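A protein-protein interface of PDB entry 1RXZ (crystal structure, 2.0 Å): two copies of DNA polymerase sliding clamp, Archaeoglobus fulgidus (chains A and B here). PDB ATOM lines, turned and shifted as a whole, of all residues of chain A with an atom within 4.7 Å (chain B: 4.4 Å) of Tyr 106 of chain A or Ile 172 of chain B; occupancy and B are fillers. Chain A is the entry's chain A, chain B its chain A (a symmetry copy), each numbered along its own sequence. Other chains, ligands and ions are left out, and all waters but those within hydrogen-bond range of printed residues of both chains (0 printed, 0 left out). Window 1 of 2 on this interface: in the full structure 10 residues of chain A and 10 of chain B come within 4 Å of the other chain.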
ATOM      1  N   ARG A  73      -2.342  21.151  21.912  1.00  0.00           N
ATOM      2  CA  ARG A  73      -2.123  20.340  20.721  1.00  0.00           C
ATOM      3  C   ARG A  73      -2.865  20.948  19.533  1.00  0.00           C
ATOM      4  O   ARG A  73      -2.384  20.893  18.398  1.00  0.00           O
ATOM      5  CB  ARG A  73      -2.607  18.913  20.982  1.00  0.00           C
ATOM      6  CG  ARG A  73      -2.043  18.329  22.268  1.00  0.00           C
ATOM      7  CD  ARG A  73      -2.606  16.947  22.595  1.00  0.00           C
ATOM      8  NE  ARG A  73      -1.804  15.834  22.073  1.00  0.00           N
ATOM      9  CZ  ARG A  73      -0.591  15.496  22.509  1.00  0.00           C
ATOM     10  NH1 ARG A  73      -0.004  16.182  23.485  1.00  0.00           N
ATOM     11  NH2 ARG A  73       0.030  14.455  21.973  1.00  0.00           N
ATOM     12  N   ILE A  77      -1.066  22.413  16.324  1.00  0.00           N
ATOM     13  CA  ILE A  77      -1.359  21.889  14.998  1.00  0.00           C
ATOM     14  C   ILE A  77      -1.794  23.029  14.097  1.00  0.00           C
ATOM     15  O   ILE A  77      -1.526  23.024  12.899  1.00  0.00           O
ATOM     16  CB  ILE A  77      -2.482  20.823  15.050  1.00  0.00           C
ATOM     17  CG1 ILE A  77      -2.687  20.188  13.671  1.00  0.00           C
ATOM     18  CG2 ILE A  77      -3.772  21.451  15.530  1.00  0.00           C
ATOM     19  CD1 ILE A  77      -3.728  20.865  12.800  1.00  0.00           C
ATOM     20  N   LEU A  97     -11.105  14.123  17.696  1.00  0.00           N
ATOM     21  CA  LEU A  97     -11.431  15.306  16.917  1.00  0.00           C
ATOM     22  C   LEU A  97     -10.601  15.333  15.642  1.00  0.00           C
ATOM     23  O   LEU A  97      -9.376  15.438  15.686  1.00  0.00           O
ATOM     24  CB  LEU A  97     -11.136  16.567  17.735  1.00  0.00           C
ATOM     25  CG  LEU A  97     -11.152  17.904  17.000  1.00  0.00           C
ATOM     26  CD1 LEU A  97     -12.582  18.351  16.757  1.00  0.00           C
ATOM     27  CD2 LEU A  97     -10.411  18.929  17.838  1.00  0.00           C
ATOM     28  N   LYS A  98     -11.280  15.230  14.506  1.00  0.00           N
ATOM     29  CA  LYS A  98     -10.623  15.262  13.211  1.00  0.00           C
ATOM     30  C   LYS A  98     -10.515  16.693  12.729  1.00  0.00           C
ATOM     31  O   LYS A  98     -11.497  17.432  12.733  1.00  0.00           O
ATOM     32  CB  LYS A  98     -11.420  14.483  12.179  1.00  0.00           C
ATOM     33  CG  LYS A  98     -11.447  12.998  12.371  1.00  0.00           C
ATOM     34  CD  LYS A  98     -12.105  12.367  11.154  1.00  0.00           C
ATOM     35  CE  LYS A  98     -12.091  10.858  11.229  1.00  0.00           C
ATOM     36  NZ  LYS A  98     -12.716  10.284  10.012  1.00  0.00           N
ATOM     37  N   VAL A  99      -9.318  17.076  12.312  1.00  0.00           N
ATOM     38  CA  VAL A  99      -9.087  18.410  11.797  1.00  0.00           C
ATOM     39  C   VAL A  99      -8.540  18.181  10.394  1.00  0.00           C
ATOM     40  O   VAL A  99      -7.456  17.616  10.228  1.00  0.00           O
ATOM     41  CB  VAL A  99      -8.058  19.179  12.661  1.00  0.00           C
ATOM     42  CG1 VAL A  99      -8.064  20.654  12.289  1.00  0.00           C
ATOM     43  CG2 VAL A  99      -8.381  19.002  14.134  1.00  0.00           C
ATOM     44  N   PHE A 101      -7.513  19.737   6.530  1.00  0.00           N
ATOM     45  CA  PHE A 101      -7.083  20.921   5.800  1.00  0.00           C
ATOM     46  C   PHE A 101      -6.024  20.538   4.779  1.00  0.00           C
ATOM     47  O   PHE A 101      -4.928  20.106   5.132  1.00  0.00           O
ATOM     48  CB  PHE A 101      -6.532  21.973   6.775  1.00  0.00           C
ATOM     49  CG  PHE A 101      -5.493  21.444   7.734  1.00  0.00           C
ATOM     50  CD1 PHE A 101      -4.130  21.637   7.488  1.00  0.00           C
ATOM     51  CD2 PHE A 101      -5.876  20.751   8.886  1.00  0.00           C
ATOM     52  CE1 PHE A 101      -3.164  21.148   8.381  1.00  0.00           C
ATOM     53  CE2 PHE A 101      -4.923  20.257   9.783  1.00  0.00           C
ATOM     54  CZ  PHE A 101      -3.565  20.456   9.531  1.00  0.00           C
ATOM     55  N   VAL A 104      -4.027  16.892   4.637  1.00  0.00           N
ATOM     56  CA  VAL A 104      -3.775  16.427   5.994  1.00  0.00           C
ATOM     57  C   VAL A 104      -5.042  16.315   6.827  1.00  0.00           C
ATOM     58  O   VAL A 104      -5.911  17.190   6.803  1.00  0.00           O
ATOM     59  CB  VAL A 104      -2.808  17.372   6.744  1.00  0.00           C
ATOM     60  CG1 VAL A 104      -2.648  16.916   8.186  1.00  0.00           C
ATOM     61  CG2 VAL A 104      -1.456  17.390   6.055  1.00  0.00           C
ATOM     62  N   GLU A 105      -5.140  15.209   7.551  1.00  0.00           N
ATOM     63  CA  GLU A 105      -6.249  14.960   8.457  1.00  0.00           C
ATOM     64  C   GLU A 105      -5.593  14.628   9.781  1.00  0.00           C
ATOM     65  O   GLU A 105      -4.988  13.571   9.935  1.00  0.00           O
ATOM     66  CB  GLU A 105      -7.099  13.781   8.000  1.00  0.00           C
ATOM     67  CG  GLU A 105      -8.134  13.370   9.027  1.00  0.00           C
ATOM     68  CD  GLU A 105      -8.966  12.170   8.592  1.00  0.00           C
ATOM     69  OE1 GLU A 105      -9.450  11.429   9.478  1.00  0.00           O
ATOM     70  OE2 GLU A 105      -9.148  11.970   7.367  1.00  0.00           O
ATOM     71  N   TYR A 106      -5.691  15.557  10.720  1.00  0.00           N
ATOM     72  CA  TYR A 106      -5.120  15.394  12.047  1.00  0.00           C
ATOM     73  C   TYR A 106      -6.210  14.902  12.996  1.00  0.00           C
ATOM     74  O   TYR A 106      -7.344  15.374  12.961  1.00  0.00           O
ATOM     75  CB  TYR A 106      -4.554  16.737  12.512  1.00  0.00           C
ATOM     76  CG  TYR A 106      -4.124  16.810  13.957  1.00  0.00           C
ATOM     77  CD1 TYR A 106      -3.122  15.985  14.453  1.00  0.00           C
ATOM     78  CD2 TYR A 106      -4.671  17.767  14.811  1.00  0.00           C
ATOM     79  CE1 TYR A 106      -2.669  16.117  15.767  1.00  0.00           C
ATOM     80  CE2 TYR A 106      -4.227  17.911  16.123  1.00  0.00           C
ATOM     81  CZ  TYR A 106      -3.222  17.086  16.598  1.00  0.00           C
ATOM     82  OH  TYR A 106      -2.764  17.244  17.894  1.00  0.00           O
ATOM     83  N   LYS A 107      -5.858  13.950  13.846  1.00  0.00           N
ATOM     84  CA  LYS A 107      -6.811  13.386  14.785  1.00  0.00           C
ATOM     85  C   LYS A 107      -6.279  13.395  16.211  1.00  0.00           C
ATOM     86  O   LYS A 107      -5.457  12.562  16.579  1.00  0.00           O
ATOM     87  CB  LYS A 107      -7.144  11.953  14.361  1.00  0.00           C
ATOM     88  CG  LYS A 107      -7.767  11.094  15.437  1.00  0.00           C
ATOM     89  CD  LYS A 107      -7.241   9.667  15.336  1.00  0.00           C
ATOM     90  CE  LYS A 107      -7.704   8.785  16.493  1.00  0.00           C
ATOM     91  NZ  LYS A 107      -9.154   8.435  16.414  1.00  0.00           N
ATOM     92  N   VAL A 108      -6.748  14.345  17.010  1.00  0.00           N
ATOM     93  CA  VAL A 108      -6.333  14.440  18.405  1.00  0.00           C
ATOM     94  C   VAL A 108      -7.478  13.931  19.281  1.00  0.00           C
ATOM     95  O   VAL A 108      -8.638  14.237  19.028  1.00  0.00           O
ATOM     96  CB  VAL A 108      -5.988  15.902  18.791  1.00  0.00           C
ATOM     97  CG1 VAL A 108      -7.161  16.813  18.485  1.00  0.00           C
ATOM     98  CG2 VAL A 108      -5.604  15.980  20.267  1.00  0.00           C
ATOM     99  N   ALA B 144       4.199  18.828   9.297  1.00  0.00           N
ATOM    100  CA  ALA B 144       3.101  18.410  10.160  1.00  0.00           C
ATOM    101  C   ALA B 144       3.449  17.197  11.033  1.00  0.00           C
ATOM    102  O   ALA B 144       3.095  17.151  12.216  1.00  0.00           O
ATOM    103  CB  ALA B 144       1.861  18.114   9.313  1.00  0.00           C
ATOM    104  N   ALA B 145       4.145  16.224  10.448  1.00  0.00           N
ATOM    105  CA  ALA B 145       4.531  14.999  11.149  1.00  0.00           C
ATOM    106  C   ALA B 145       5.544  15.239  12.254  1.00  0.00           C
ATOM    107  O   ALA B 145       5.636  14.468  13.200  1.00  0.00           O
ATOM    108  CB  ALA B 145       5.094  14.003  10.157  1.00  0.00           C
ATOM    109  N   ILE B 148       4.065  15.660  15.660  1.00  0.00           N
ATOM    110  CA  ILE B 148       3.529  14.443  16.245  1.00  0.00           C
ATOM    111  C   ILE B 148       4.615  13.438  16.628  1.00  0.00           C
ATOM    112  O   ILE B 148       4.523  12.791  17.681  1.00  0.00           O
ATOM    113  CB  ILE B 148       2.494  13.750  15.279  1.00  0.00           C
ATOM    114  CG1 ILE B 148       1.238  14.616  15.120  1.00  0.00           C
ATOM    115  CG2 ILE B 148       2.054  12.411  15.844  1.00  0.00           C
ATOM    116  CD1 ILE B 148       1.460  15.903  14.384  1.00  0.00           C
ATOM    117  N   ILE B 163       1.467   9.180   4.190  1.00  0.00           N
ATOM    118  CA  ILE B 163       2.567   9.514   5.088  1.00  0.00           C
ATOM    119  C   ILE B 163       1.858   9.682   6.442  1.00  0.00           C
ATOM    120  O   ILE B 163       0.948  10.502   6.576  1.00  0.00           O
ATOM    121  CB  ILE B 163       3.272  10.832   4.645  1.00  0.00           C
ATOM    122  CG1 ILE B 163       3.606  10.769   3.150  1.00  0.00           C
ATOM    123  CG2 ILE B 163       4.552  11.038   5.439  1.00  0.00           C
ATOM    124  CD1 ILE B 163       4.418  11.943   2.649  1.00  0.00           C
ATOM    125  N   GLU B 164       2.253   8.890   7.437  1.00  0.00           N
ATOM    126  CA  GLU B 164       1.608   8.949   8.751  1.00  0.00           C
ATOM    127  C   GLU B 164       2.548   9.103   9.950  1.00  0.00           C
ATOM    128  O   GLU B 164       3.666   8.579   9.962  1.00  0.00           O
ATOM    129  CB  GLU B 164       0.768   7.696   8.957  1.00  0.00           C
ATOM    130  CG  GLU B 164       0.015   7.275   7.723  1.00  0.00           C
ATOM    131  CD  GLU B 164      -0.038   5.773   7.581  1.00  0.00           C
ATOM    132  OE1 GLU B 164      -0.626   5.112   8.459  1.00  0.00           O
ATOM    133  OE2 GLU B 164       0.520   5.256   6.591  1.00  0.00           O
ATOM    134  N   ALA B 165       2.063   9.811  10.965  1.00  0.00           N
ATOM    135  CA  ALA B 165       2.816  10.042  12.195  1.00  0.00           C
ATOM    136  C   ALA B 165       1.879   9.876  13.389  1.00  0.00           C
ATOM    137  O   ALA B 165       0.737  10.329  13.365  1.00  0.00           O
ATOM    138  CB  ALA B 165       3.428  11.447  12.188  1.00  0.00           C
ATOM    139  N   ASP B 170      -2.285  11.894  19.795  1.00  0.00           N
ATOM    140  CA  ASP B 170      -2.758  12.343  18.491  1.00  0.00           C
ATOM    141  C   ASP B 170      -2.062  11.636  17.332  1.00  0.00           C
ATOM    142  O   ASP B 170      -1.091  10.917  17.528  1.00  0.00           O
ATOM    143  CB  ASP B 170      -2.574  13.859  18.363  1.00  0.00           C
ATOM    144  CG  ASP B 170      -1.159  14.314  18.698  1.00  0.00           C
ATOM    145  OD1 ASP B 170      -0.927  15.545  18.776  1.00  0.00           O
ATOM    146  OD2 ASP B 170      -0.278  13.447  18.883  1.00  0.00           O
ATOM    147  N   SER B 171      -2.581  11.837  16.125  1.00  0.00           N
ATOM    148  CA  SER B 171      -2.020  11.235  14.918  1.00  0.00           C
ATOM    149  C   SER B 171      -2.358  12.105  13.712  1.00  0.00           C
ATOM    150  O   SER B 171      -3.310  12.884  13.738  1.00  0.00           O
ATOM    151  CB  SER B 171      -2.570   9.817  14.714  1.00  0.00           C
ATOM    152  OG  SER B 171      -3.980   9.811  14.576  1.00  0.00           O
ATOM    153  N   ILE B 172      -1.575  11.965  12.652  1.00  0.00           N
ATOM    154  CA  ILE B 172      -1.784  12.758  11.455  1.00  0.00           C
ATOM    155  C   ILE B 172      -1.501  11.894  10.224  1.00  0.00           C
ATOM    156  O   ILE B 172      -0.657  11.000  10.270  1.00  0.00           O
ATOM    157  CB  ILE B 172      -0.857  13.997  11.496  1.00  0.00           C
ATOM    158  CG1 ILE B 172      -1.591  15.213  10.965  1.00  0.00           C
ATOM    159  CG2 ILE B 172       0.408  13.750  10.701  1.00  0.00           C
ATOM    160  CD1 ILE B 172      -0.909  16.513  11.313  1.00  0.00           C
ATOM    161  N   VAL B 173      -2.232  12.129   9.136  1.00  0.00           N
ATOM    162  CA  VAL B 173      -2.011  11.373   7.910  1.00  0.00           C
ATOM    163  C   VAL B 173      -2.167  12.270   6.699  1.00  0.00           C
ATOM    164  O   VAL B 173      -3.140  13.022   6.575  1.00  0.00           O
ATOM    165  CB  VAL B 173      -2.990  10.184   7.748  1.00  0.00           C
ATOM    166  CG1 VAL B 173      -2.618   9.379   6.515  1.00  0.00           C
ATOM    167  CG2 VAL B 173      -2.949   9.297   8.961  1.00  0.00           C
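The guanidinium group of Arg 73 of chain A is in salt-bridge range of the side-chain carboxylate of Asp 170 of chain B (3.3 Å).
The backbone carbonyl oxygen (O) of Val 173 of chain B sits at hydrogen-bond distance from the backbone NH (N) of Glu 105 of chain A.
The side-chain carboxylate (OD1) of Asp 170 of chain B sits at hydrogen-bond distance from the side-chain hydroxyl (OH) of Tyr 106 of chain A.
N of Lys 107 of chain A is in hydrogen-bond range of O of Ser 171 of chain B (2.8 Å).
O of Val 108 of chain A lies within hydrogen-bond range of N of Leu 97 of chain A, at 2.8 Å.
The side-chain carboxylate (OE1) of Glu 105 of chain A lies within salt-bridge range of the side-chain amino group (NZ) of Lys 98 of chain A (3.5 Å).
N of Val 99 of chain A is in hydrogen-bond range of O of Tyr 106 of chain A, 2.7 Å away.
The backbone NH (N) of Ile 172 of chain B is in hydrogen-bond range of the backbone carbonyl oxygen (O) of Ala 165 of chain B, 2.9 Å away.
Among the printed residues, merely in contact across the chains: Val 104 of chain A with Ile 172 of chain B (3.4 Å), Val 104 of chain A with Val 173 of chain B (3.5 Å), Glu 105 of chain A with Ile 172 of chain B (3.6 Å), Tyr 106 of chain A with Ser 171 of chain B (3.2 Å), Tyr 106 of chain A with Ile 172 of chain B (3.7 Å), Lys 107 of chain A with Asp 170 of chain B (3.3 Å) and Val 108 of chain A with Asp 170 of chain B (3.8 Å).
Tyr 106 of chain A touches just these residues of chain B: Asp 170 (2.7 Å), Ser 171 (3.2 Å) and Ile 172 (3.7 Å).
Ile 172 of chain B touches three residues of chain A.
Of the printed residues of chain B, Glu 105 of chain A touches Ile 172 and Val 173.
Printed residues of chain B within 4 Å of Val 104 of chain A: Ile 172 and Val 173.
Printed residues of chain A within 4 Å of Asp 170 of chain B: Arg 73 (3.3 Å), Tyr 106 (2.7 Å), Lys 107 (3.3 Å) and Val 108 (3.8 Å).
Ala 165 of chain B touches none of the printed residues of chain A.
Lys 98 of chain A touches none of the printed residues of chain B.
The nearest residue of chain B that does not touch Tyr 106 of chain A is Ile 148 of chain B (4.2 Å).
The nearest printed residue of chain A that does not touch Ile 172 of chain B is Ile 77 of chain A (4.7 Å).
Hydrophobic or aromatic side chains of chain A that line the printed part of chain B: Val 104 and Tyr 106.
Hydrophobic or aromatic side chains of chain B that line the printed part of chain A: Ile 172.
Among the printed residues, Asp or Glu carboxylates within 4 Å of a Lys or Arg side-chain nitrogen of the other chain: Arg 73 of chain A with Asp 170 of chain B (3.3 Å).
No position is printed for both chains.
Of the 11 pairs that touch across the chains among the printed residues, none has its exchanged pair printed and touching as well.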
